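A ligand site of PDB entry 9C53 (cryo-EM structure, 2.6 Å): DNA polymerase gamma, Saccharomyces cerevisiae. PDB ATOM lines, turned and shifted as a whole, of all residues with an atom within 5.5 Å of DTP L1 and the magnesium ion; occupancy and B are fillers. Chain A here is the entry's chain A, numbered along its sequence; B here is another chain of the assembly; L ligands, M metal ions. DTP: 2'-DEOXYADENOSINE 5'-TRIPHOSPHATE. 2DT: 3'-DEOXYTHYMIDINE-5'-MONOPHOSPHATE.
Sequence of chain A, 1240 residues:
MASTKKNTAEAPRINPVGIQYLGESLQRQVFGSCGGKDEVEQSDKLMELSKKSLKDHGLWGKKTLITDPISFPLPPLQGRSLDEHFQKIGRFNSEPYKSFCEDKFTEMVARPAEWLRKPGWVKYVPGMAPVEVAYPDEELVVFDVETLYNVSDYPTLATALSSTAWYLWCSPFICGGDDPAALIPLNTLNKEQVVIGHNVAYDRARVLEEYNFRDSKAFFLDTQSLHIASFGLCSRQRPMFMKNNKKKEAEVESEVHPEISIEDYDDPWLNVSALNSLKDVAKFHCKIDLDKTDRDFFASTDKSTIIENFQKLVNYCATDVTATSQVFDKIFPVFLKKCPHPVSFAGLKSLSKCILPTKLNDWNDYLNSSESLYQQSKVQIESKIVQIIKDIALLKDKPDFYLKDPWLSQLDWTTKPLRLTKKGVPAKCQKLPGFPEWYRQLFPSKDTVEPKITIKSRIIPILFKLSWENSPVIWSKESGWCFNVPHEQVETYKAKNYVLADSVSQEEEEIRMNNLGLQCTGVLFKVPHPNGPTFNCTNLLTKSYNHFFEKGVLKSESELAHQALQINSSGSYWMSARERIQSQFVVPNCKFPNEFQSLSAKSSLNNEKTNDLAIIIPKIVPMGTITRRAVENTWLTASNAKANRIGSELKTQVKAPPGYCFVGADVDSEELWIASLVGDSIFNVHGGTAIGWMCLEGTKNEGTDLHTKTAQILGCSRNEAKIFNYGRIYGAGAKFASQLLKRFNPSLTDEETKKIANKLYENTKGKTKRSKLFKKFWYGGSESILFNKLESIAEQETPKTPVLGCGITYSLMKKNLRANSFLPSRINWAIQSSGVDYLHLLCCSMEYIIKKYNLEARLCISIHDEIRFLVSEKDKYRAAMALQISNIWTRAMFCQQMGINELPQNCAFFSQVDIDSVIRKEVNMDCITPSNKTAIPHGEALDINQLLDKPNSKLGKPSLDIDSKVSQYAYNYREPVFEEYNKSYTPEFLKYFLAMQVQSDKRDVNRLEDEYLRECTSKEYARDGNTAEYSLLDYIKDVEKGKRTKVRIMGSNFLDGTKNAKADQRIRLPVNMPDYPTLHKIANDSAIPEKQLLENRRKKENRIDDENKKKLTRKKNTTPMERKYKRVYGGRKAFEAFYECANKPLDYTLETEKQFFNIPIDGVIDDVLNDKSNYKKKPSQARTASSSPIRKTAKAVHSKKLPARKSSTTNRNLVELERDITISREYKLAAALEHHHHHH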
ATOM      1  N   ARG A 629      -6.863 -11.715  -9.592  1.00  0.00           N
ATOM      2  CA  ARG A 629      -5.876 -10.667  -9.777  1.00  0.00           C
ATOM      3  C   ARG A 629      -6.120  -9.941 -11.091  1.00  0.00           C
ATOM      4  O   ARG A 629      -6.747 -10.475 -12.006  1.00  0.00           O
ATOM      5  CB  ARG A 629      -4.446 -11.222  -9.742  1.00  0.00           C
ATOM      6  CG  ARG A 629      -4.139 -12.084  -8.529  1.00  0.00           C
ATOM      7  CD  ARG A 629      -2.726 -11.833  -8.019  1.00  0.00           C
ATOM      8  NE  ARG A 629      -1.709 -12.283  -8.969  1.00  0.00           N
ATOM      9  CZ  ARG A 629      -0.422 -12.373  -8.689  1.00  0.00           C
ATOM     10  NH1 ARG A 629       0.060 -12.067  -7.494  1.00  0.00           N
ATOM     11  NH2 ARG A 629       0.422 -12.771  -9.646  1.00  0.00           N
ATOM     12  N   ASP A 666       5.489   0.157  -1.180  1.00  0.00           N
ATOM     13  CA  ASP A 666       5.450  -1.285  -1.554  1.00  0.00           C
ATOM     14  C   ASP A 666       5.482  -2.158  -0.300  1.00  0.00           C
ATOM     15  O   ASP A 666       6.219  -1.805   0.642  1.00  0.00           O
ATOM     16  CB  ASP A 666       6.622  -1.650  -2.475  1.00  0.00           C
ATOM     17  CG  ASP A 666       6.424  -2.955  -3.233  1.00  0.00           C
ATOM     18  OD1 ASP A 666       7.026  -3.963  -2.829  1.00  0.00           O
ATOM     19  OD2 ASP A 666       5.683  -2.944  -4.231  1.00  0.00           O
ATOM     20  N   VAL A 667       4.721  -3.253  -0.275  1.00  0.00           N
ATOM     21  CA  VAL A 667       4.644  -4.163   0.920  1.00  0.00           C
ATOM     22  C   VAL A 667       5.936  -4.969   1.048  1.00  0.00           C
ATOM     23  O   VAL A 667       6.596  -5.184   0.012  1.00  0.00           O
ATOM     24  CB  VAL A 667       3.394  -5.069   0.868  1.00  0.00           C
ATOM     25  CG1 VAL A 667       3.108  -5.725   2.209  1.00  0.00           C
ATOM     26  CG2 VAL A 667       2.173  -4.320   0.362  1.00  0.00           C
ATOM     27  N   ASP A 668       6.290  -5.409   2.259  1.00  0.00           N
ATOM     28  CA  ASP A 668       7.571  -6.136   2.489  1.00  0.00           C
ATOM     29  C   ASP A 668       7.311  -7.591   2.893  1.00  0.00           C
ATOM     30  O   ASP A 668       6.556  -7.796   3.854  1.00  0.00           O
ATOM     31  CB  ASP A 668       8.400  -5.418   3.550  1.00  0.00           C
ATOM     32  CG  ASP A 668       8.491  -3.921   3.340  1.00  0.00           C
ATOM     33  OD1 ASP A 668       8.620  -3.498   2.175  1.00  0.00           O
ATOM     34  OD2 ASP A 668       8.423  -3.181   4.342  1.00  0.00           O
ATOM     35  N   SER A 669       7.907  -8.557   2.177  1.00  0.00           N
ATOM     36  CA  SER A 669       7.765 -10.004   2.510  1.00  0.00           C
ATOM     37  C   SER A 669       6.274 -10.344   2.654  1.00  0.00           C
ATOM     38  O   SER A 669       5.924 -10.961   3.668  1.00  0.00           O
ATOM     39  CB  SER A 669       8.544 -10.351   3.746  1.00  0.00           C
ATOM     40  OG  SER A 669       9.937 -10.194   3.508  1.00  0.00           O
ATOM     41  N   GLU A 670       5.460  -9.965   1.676  1.00  0.00           N
ATOM     42  CA  GLU A 670       3.980 -10.117   1.814  1.00  0.00           C
ATOM     43  C   GLU A 670       3.504 -11.566   1.947  1.00  0.00           C
ATOM     44  O   GLU A 670       2.701 -11.817   2.860  1.00  0.00           O
ATOM     45  CB  GLU A 670       3.311  -9.493   0.583  1.00  0.00           C
ATOM     46  CG  GLU A 670       1.827  -9.237   0.778  1.00  0.00           C
ATOM     47  CD  GLU A 670       1.066  -9.021  -0.522  1.00  0.00           C
ATOM     48  OE1 GLU A 670       1.377  -9.712  -1.503  1.00  0.00           O
ATOM     49  OE2 GLU A 670       0.162  -8.169  -0.540  1.00  0.00           O
ATOM     50  N   GLU A 671       3.997 -12.501   1.134  1.00  0.00           N
ATOM     51  CA  GLU A 671       3.414 -13.879   1.155  1.00  0.00           C
ATOM     52  C   GLU A 671       4.125 -14.756   2.190  1.00  0.00           C
ATOM     53  O   GLU A 671       3.580 -15.810   2.521  1.00  0.00           O
ATOM     54  CB  GLU A 671       3.455 -14.479  -0.254  1.00  0.00           C
ATOM     55  CG  GLU A 671       2.207 -14.152  -1.056  1.00  0.00           C
ATOM     56  CD  GLU A 671       2.114 -14.816  -2.419  1.00  0.00           C
ATOM     57  OE1 GLU A 671       2.300 -16.054  -2.492  1.00  0.00           O
ATOM     58  OE2 GLU A 671       1.866 -14.099  -3.410  1.00  0.00           O
ATOM     59  N   LYS A 700      14.441  -4.884   7.442  1.00  0.00           N
ATOM     60  CA  LYS A 700      15.136  -4.651   6.190  1.00  0.00           C
ATOM     61  C   LYS A 700      16.079  -3.454   6.275  1.00  0.00           C
ATOM     62  O   LYS A 700      17.138  -3.442   5.617  1.00  0.00           O
ATOM     63  CB  LYS A 700      14.135  -4.457   5.046  1.00  0.00           C
ATOM     64  CG  LYS A 700      14.765  -4.560   3.668  1.00  0.00           C
ATOM     65  CD  LYS A 700      13.821  -4.062   2.588  1.00  0.00           C
ATOM     66  CE  LYS A 700      12.686  -5.041   2.360  1.00  0.00           C
ATOM     67  NZ  LYS A 700      11.855  -4.668   1.183  1.00  0.00           N
ATOM     68  N   HIS A 707      15.515 -12.872   3.675  1.00  0.00           N
ATOM     69  CA  HIS A 707      15.972 -13.000   2.299  1.00  0.00           C
ATOM     70  C   HIS A 707      17.442 -12.612   2.179  1.00  0.00           C
ATOM     71  O   HIS A 707      18.207 -13.273   1.456  1.00  0.00           O
ATOM     72  CB  HIS A 707      15.114 -12.139   1.376  1.00  0.00           C
ATOM     73  CG  HIS A 707      13.772 -12.734   1.061  1.00  0.00           C
ATOM     74  ND1 HIS A 707      13.624 -14.047   0.668  1.00  0.00           N
ATOM     75  CD2 HIS A 707      12.531 -12.198   1.072  1.00  0.00           C
ATOM     76  CE1 HIS A 707      12.346 -14.295   0.457  1.00  0.00           C
ATOM     77  NE2 HIS A 707      11.664 -13.191   0.697  1.00  0.00           N
ATOM     78  N   ARG A 718      19.680 -10.829  -3.881  1.00  0.00           N
ATOM     79  CA  ARG A 718      18.475 -10.952  -3.052  1.00  0.00           C
ATOM     80  C   ARG A 718      17.289 -11.473  -3.869  1.00  0.00           C
ATOM     81  O   ARG A 718      16.455 -12.223  -3.336  1.00  0.00           O
ATOM     82  CB  ARG A 718      18.144  -9.604  -2.418  1.00  0.00           C
ATOM     83  CG  ARG A 718      17.377  -9.701  -1.105  1.00  0.00           C
ATOM     84  CD  ARG A 718      16.830  -8.353  -0.700  1.00  0.00           C
ATOM     85  NE  ARG A 718      15.832  -8.454   0.366  1.00  0.00           N
ATOM     86  CZ  ARG A 718      14.553  -8.150   0.216  1.00  0.00           C
ATOM     87  NH1 ARG A 718      14.068  -7.721  -0.928  1.00  0.00           N
ATOM     88  NH2 ARG A 718      13.736  -8.289   1.258  1.00  0.00           N
ATOM     89  N   LYS A 722      14.991 -14.752  -3.203  1.00  0.00           N
ATOM     90  CA  LYS A 722      13.534 -14.754  -3.157  1.00  0.00           C
ATOM     91  C   LYS A 722      12.963 -15.857  -4.041  1.00  0.00           C
ATOM     92  O   LYS A 722      12.015 -16.549  -3.654  1.00  0.00           O
ATOM     93  CB  LYS A 722      12.984 -13.399  -3.591  1.00  0.00           C
ATOM     94  CG  LYS A 722      12.881 -12.385  -2.467  1.00  0.00           C
ATOM     95  CD  LYS A 722      12.044 -11.180  -2.883  1.00  0.00           C
ATOM     96  CE  LYS A 722      12.588 -10.515  -4.133  1.00  0.00           C
ATOM     97  NZ  LYS A 722      11.723  -9.398  -4.586  1.00  0.00           N
ATOM     98  N   ILE A 723      13.541 -16.042  -5.229  1.00  0.00           N
ATOM     99  CA  ILE A 723      13.111 -17.123  -6.131  1.00  0.00           C
ATOM    100  C   ILE A 723      13.345 -18.478  -5.477  1.00  0.00           C
ATOM    101  O   ILE A 723      12.477 -19.360  -5.509  1.00  0.00           O
ATOM    102  CB  ILE A 723      13.836 -17.011  -7.486  1.00  0.00           C
ATOM    103  CG1 ILE A 723      13.464 -15.707  -8.194  1.00  0.00           C
ATOM    104  CG2 ILE A 723      13.504 -18.210  -8.367  1.00  0.00           C
ATOM    105  CD1 ILE A 723      14.212 -15.484  -9.478  1.00  0.00           C
ATOM    106  N   TYR A 726      10.710 -18.960  -2.561  1.00  0.00           N
ATOM    107  CA  TYR A 726       9.342 -19.171  -3.008  1.00  0.00           C
ATOM    108  C   TYR A 726       9.182 -20.461  -3.794  1.00  0.00           C
ATOM    109  O   TYR A 726       8.096 -21.040  -3.831  1.00  0.00           O
ATOM    110  CB  TYR A 726       8.858 -17.975  -3.823  1.00  0.00           C
ATOM    111  CG  TYR A 726       8.557 -16.761  -2.977  1.00  0.00           C
ATOM    112  CD1 TYR A 726       7.824 -16.870  -1.806  1.00  0.00           C
ATOM    113  CD2 TYR A 726       9.015 -15.507  -3.347  1.00  0.00           C
ATOM    114  CE1 TYR A 726       7.548 -15.767  -1.019  1.00  0.00           C
ATOM    115  CE2 TYR A 726       8.749 -14.389  -2.577  1.00  0.00           C
ATOM    116  CZ  TYR A 726       8.011 -14.535  -1.412  1.00  0.00           C
ATOM    117  OH  TYR A 726       7.740 -13.425  -0.640  1.00  0.00           O
ATOM    118  N   GLY A 727      10.257 -20.922  -4.439  1.00  0.00           N
ATOM    119  CA  GLY A 727      10.220 -22.256  -5.030  1.00  0.00           C
ATOM    120  C   GLY A 727      10.162 -23.354  -3.993  1.00  0.00           C
ATOM    121  O   GLY A 727       9.533 -24.392  -4.229  1.00  0.00           O
ATOM    122  N   TYR A 730       6.426 -23.710  -2.181  1.00  0.00           N
ATOM    123  CA  TYR A 730       5.623 -24.593  -3.000  1.00  0.00           C
ATOM    124  C   TYR A 730       6.436 -25.840  -3.353  1.00  0.00           C
ATOM    125  O   TYR A 730       7.599 -25.981  -2.978  1.00  0.00           O
ATOM    126  CB  TYR A 730       5.133 -23.859  -4.243  1.00  0.00           C
ATOM    127  CG  TYR A 730       4.510 -22.522  -3.895  1.00  0.00           C
ATOM    128  CD1 TYR A 730       3.500 -22.434  -2.939  1.00  0.00           C
ATOM    129  CD2 TYR A 730       4.931 -21.356  -4.502  1.00  0.00           C
ATOM    130  CE1 TYR A 730       2.934 -21.214  -2.607  1.00  0.00           C
ATOM    131  CE2 TYR A 730       4.375 -20.133  -4.178  1.00  0.00           C
ATOM    132  CZ  TYR A 730       3.367 -20.073  -3.229  1.00  0.00           C
ATOM    133  OH  TYR A 730       2.812 -18.863  -2.898  1.00  0.00           O
ATOM    134  N   ASP A 865       0.783  -5.351  -4.947  1.00  0.00           N
ATOM    135  CA  ASP A 865       1.645  -5.075  -3.752  1.00  0.00           C
ATOM    136  C   ASP A 865       2.242  -3.651  -3.820  1.00  0.00           C
ATOM    137  O   ASP A 865       2.937  -3.274  -2.864  1.00  0.00           O
ATOM    138  CB  ASP A 865       2.650  -6.217  -3.531  1.00  0.00           C
ATOM    139  CG  ASP A 865       4.109  -5.818  -3.484  1.00  0.00           C
ATOM    140  OD1 ASP A 865       4.725  -5.687  -4.563  1.00  0.00           O
ATOM    141  OD2 ASP A 865       4.640  -5.658  -2.366  1.00  0.00           O
ATOM    142  P    DT B  18       9.568 -28.854 -10.306  1.00  0.00           P
ATOM    143  OP1  DT B  18       9.832 -28.535 -11.722  1.00  0.00           O
ATOM    144  OP2  DT B  18      10.645 -29.456  -9.490  1.00  0.00           O
ATOM    145  O5'  DT B  18       9.067 -27.539  -9.548  1.00  0.00           O
ATOM    146  C5'  DT B  18       8.034 -26.723 -10.124  1.00  0.00           C
ATOM    147  C4'  DT B  18       7.279 -25.985  -9.046  1.00  0.00           C
ATOM    148  O4'  DT B  18       8.160 -25.048  -8.385  1.00  0.00           O
ATOM    149  C3'  DT B  18       6.129 -25.123  -9.545  1.00  0.00           C
ATOM    150  O3'  DT B  18       4.957 -25.912  -9.691  1.00  0.00           O
ATOM    151  C2'  DT B  18       5.976 -24.105  -8.412  1.00  0.00           C
ATOM    152  C1'  DT B  18       7.424 -23.927  -7.927  1.00  0.00           C
ATOM    153  N1   DT B  18       8.068 -22.683  -8.438  1.00  0.00           N
ATOM    154  C2   DT B  18       7.741 -21.468  -7.874  1.00  0.00           C
ATOM    155  O2   DT B  18       6.937 -21.351  -6.968  1.00  0.00           O
ATOM    156  N3   DT B  18       8.396 -20.394  -8.404  1.00  0.00           N
ATOM    157  C4   DT B  18       9.319 -20.408  -9.426  1.00  0.00           C
ATOM    158  O4   DT B  18       9.852 -19.384  -9.847  1.00  0.00           O
ATOM    159  C5   DT B  18       9.622 -21.706  -9.977  1.00  0.00           C
ATOM    160  C7   DT B  18      10.612 -21.844 -11.093  1.00  0.00           C
ATOM    161  C6   DT B  18       8.989 -22.775  -9.465  1.00  0.00           C
ATOM    162  P    DA B  19       3.891 -25.573 -10.841  1.00  0.00           P
ATOM    163  OP1  DA B  19       2.912 -26.680 -10.885  1.00  0.00           O
ATOM    164  OP2  DA B  19       4.635 -25.204 -12.062  1.00  0.00           O
ATOM    165  O5'  DA B  19       3.144 -24.260 -10.314  1.00  0.00           O
ATOM    166  C5'  DA B  19       2.200 -24.354  -9.250  1.00  0.00           C
ATOM    167  C4'  DA B  19       1.695 -22.977  -8.853  1.00  0.00           C
ATOM    168  O4'  DA B  19       2.780 -22.196  -8.325  1.00  0.00           O
ATOM    169  C3'  DA B  19       1.144 -22.136 -10.001  1.00  0.00           C
ATOM    170  O3'  DA B  19      -0.221 -22.459 -10.224  1.00  0.00           O
ATOM    171  C2'  DA B  19       1.297 -20.723  -9.460  1.00  0.00           C
ATOM    172  C1'  DA B  19       2.556 -20.823  -8.586  1.00  0.00           C
ATOM    173  N9   DA B  19       3.746 -20.256  -9.206  1.00  0.00           N
ATOM    174  C8   DA B  19       4.850 -20.929  -9.629  1.00  0.00           C
ATOM    175  N7   DA B  19       5.776 -20.149 -10.157  1.00  0.00           N
ATOM    176  C5   DA B  19       5.226 -18.878 -10.065  1.00  0.00           C
ATOM    177  C6   DA B  19       5.707 -17.618 -10.440  1.00  0.00           C
ATOM    178  N6   DA B  19       6.905 -17.419 -11.011  1.00  0.00           N
ATOM    179  N1   DA B  19       4.914 -16.554 -10.208  1.00  0.00           N
ATOM    180  C2   DA B  19       3.723 -16.745  -9.638  1.00  0.00           C
ATOM    181  N3   DA B  19       3.164 -17.882  -9.238  1.00  0.00           N
ATOM    182  C4   DA B  19       3.980 -18.929  -9.481  1.00  0.00           C
HETATM  183  PG  DTP L   1       9.929  -7.353  -1.013  1.00  0.00           P
HETATM  184  O1G DTP L   1      11.063  -7.166  -1.982  1.00  0.00           O
HETATM  185  O2G DTP L   1       8.744  -6.486  -1.341  1.00  0.00           O
HETATM  186  O3G DTP L   1      10.358  -7.225   0.418  1.00  0.00           O
HETATM  187  PB  DTP L   1       8.057  -9.586  -1.569  1.00  0.00           P
HETATM  188  O1B DTP L   1       6.933  -8.665  -1.269  1.00  0.00           O
HETATM  189  O2B DTP L   1       8.051 -10.964  -1.002  1.00  0.00           O
HETATM  190  O3B DTP L   1       9.442  -8.881  -1.170  1.00  0.00           O
HETATM  191  PA  DTP L   1       7.690  -8.837  -4.398  1.00  0.00           P
HETATM  192  O1A DTP L   1       7.737  -7.394  -4.048  1.00  0.00           O
HETATM  193  O2A DTP L   1       8.407  -9.279  -5.627  1.00  0.00           O
HETATM  194  O3A DTP L   1       8.233  -9.695  -3.155  1.00  0.00           O
HETATM  195  O5' DTP L   1       6.173  -9.321  -4.462  1.00  0.00           O
HETATM  196  C5' DTP L   1       5.825 -10.362  -5.422  1.00  0.00           C
HETATM  197  C4' DTP L   1       4.686 -11.183  -4.877  1.00  0.00           C
HETATM  198  O4' DTP L   1       4.502 -12.340  -5.705  1.00  0.00           O
HETATM  199  C3' DTP L   1       4.903 -11.709  -3.454  1.00  0.00           C
HETATM  200  O3' DTP L   1       3.654 -11.864  -2.796  1.00  0.00           O
HETATM  201  C2' DTP L   1       5.577 -13.059  -3.703  1.00  0.00           C
HETATM  202  C1' DTP L   1       5.099 -13.479  -5.083  1.00  0.00           C
HETATM  203  N9  DTP L   1       6.188 -13.949  -5.945  1.00  0.00           N
HETATM  204  C8  DTP L   1       7.160 -13.193  -6.538  1.00  0.00           C
HETATM  205  N7  DTP L   1       7.997 -13.914  -7.251  1.00  0.00           N
HETATM  206  C5  DTP L   1       7.556 -15.218  -7.098  1.00  0.00           C
HETATM  207  C6  DTP L   1       8.010 -16.450  -7.597  1.00  0.00           C
HETATM  208  N6  DTP L   1       9.081 -16.575  -8.384  1.00  0.00           N
HETATM  209  N1  DTP L   1       7.326 -17.557  -7.255  1.00  0.00           N
HETATM  210  C2  DTP L   1       6.251 -17.427  -6.461  1.00  0.00           C
HETATM  211  N3  DTP L   1       5.725 -16.327  -5.932  1.00  0.00           N
HETATM  212  C4  DTP L   1       6.432 -15.243  -6.299  1.00  0.00           C
HETATM  213  P   2DT L   2       8.427  -6.737  -9.988  1.00  0.00           P
HETATM  214  OP1 2DT L   2       8.126  -5.321 -10.381  1.00  0.00           O
HETATM  215  OP2 2DT L   2       9.441  -7.307 -10.957  1.00  0.00           O
HETATM  216  O5' 2DT L   2       7.047  -7.615 -10.061  1.00  0.00           O
HETATM  217  N1  2DT L   2       5.217 -10.996 -10.242  1.00  0.00           N
HETATM  218  C6  2DT L   2       6.507 -10.714 -10.803  1.00  0.00           C
HETATM  219  C2  2DT L   2       4.860 -12.380  -9.830  1.00  0.00           C
HETATM  220  O2  2DT L   2       3.791 -12.616  -9.374  1.00  0.00           O
HETATM  221  N3  2DT L   2       5.848 -13.481 -10.001  1.00  0.00           N
HETATM  222  C4  2DT L   2       7.161 -13.194 -10.565  1.00  0.00           C
HETATM  223  O4  2DT L   2       7.949 -14.065 -10.699  1.00  0.00           O
HETATM  224  C5  2DT L   2       7.504 -11.795 -10.969  1.00  0.00           C
HETATM  225  C5M 2DT L   2       8.873 -11.493 -11.565  1.00  0.00           C
HETATM  226  C2' 2DT L   2       4.239  -9.387  -8.554  1.00  0.00           C
HETATM  227  C5' 2DT L   2       5.852  -6.937 -10.305  1.00  0.00           C
HETATM  228  C4' 2DT L   2       4.747  -7.705  -9.903  1.00  0.00           C
HETATM  229  O4' 2DT L   2       4.560  -8.931 -10.844  1.00  0.00           O
HETATM  230  C1' 2DT L   2       4.248  -9.926 -10.081  1.00  0.00           C
HETATM  231  C3' 2DT L   2       4.971  -8.324  -8.523  1.00  0.00           C
HETATM  232 MG    MG M   1       6.613  -6.204  -1.744  1.00  0.00          MG
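Three residues have an atom within 4 Å of the magnesium ion: Asp 666, Val 667 and Asp 865. Along chain A the residues within 4 Å of the magnesium ion span positions 666 to 865.
Asp 668 touches DTP L1 (CA to O3G, 3.6 Å). N6 of DA 19 of chain B touches N6 of DTP L1 (3.5 Å). Hydrophobic or aromatic side chains within 4 Å of DTP L1: Tyr 726. Within 4 Å of DTP L1: Asp 666, Val 667, Asp 668, Ser 669, Glu 670, Glu 671, Lys 700, Arg 718, Lys 722, Tyr 726, Asp 865, DT 18 of chain B and DA 19 of chain B. Along chain A the residues within 4 Å of DTP L1 span positions 666 to 865. The nearest printed residue that does not touch DTP L1 is Tyr 730 (4.01 Å).
The magnesium ion is bound by the backbone carbonyl oxygen of Val 667 (2.0 Å), the side-chain carboxylate of Asp 865 (2.1 Å), an oxygen (O2G) of DTP L1 (2.2 Å), the side-chain carboxylate of Asp 666 (2.5 Å) and an oxygen (O1B) of DTP L1 (2.5 Å). The magnesium ion has five donor atoms within binding distance. Slightly farther from the magnesium ion lies an oxygen (O1A) of DTP L1 (2.8 Å).
The side-chain amino group (NZ) of Lys 700 is in salt-bridge range of the side-chain carboxylate (OD1) of Asp 668 (3.6 Å). The side-chain hydroxyl (OH) of Tyr 730 lies within hydrogen-bond range of the side-chain carboxylate (OE1) of Glu 671 (2.9 Å).
The guanidinium group of Arg 629 sits at hydrogen-bond distance from an oxygen (O2) of 2DT L2 (3.4 Å). O4 of DT 18 of chain B lies within hydrogen-bond range of a nitrogen (N6) of DTP L1, 3.3 Å away. OH of Tyr 726 is in hydrogen-bond range of O2B of DTP L1, at 2.5 Å. The side-chain carboxylate of Glu 670 lies within hydrogen-bond range of an oxygen (O3') of DTP L1, at 3.4 Å. NZ of Lys 700 lies within salt-bridge range of O3G of DTP L1 (3.1 Å). An oxygen (O3G) of DTP L1 sits at hydrogen-bond distance from the backbone NH of Ser 669 (3.3 Å). NZ of Lys 722 is in salt-bridge range of O2A of DTP L1, 3.5 Å away. The guanidinium group (NH1) of Arg 718 is in salt-bridge range of an oxygen (O1G) of DTP L1 (3.2 Å). N1 of DA 19 of chain B sits at hydrogen-bond distance from a nitrogen (N3) of 2DT L2. An oxygen (O3') of DTP L1 sits at hydrogen-bond distance from the side-chain carboxylate of Glu 671 (2.9 Å).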
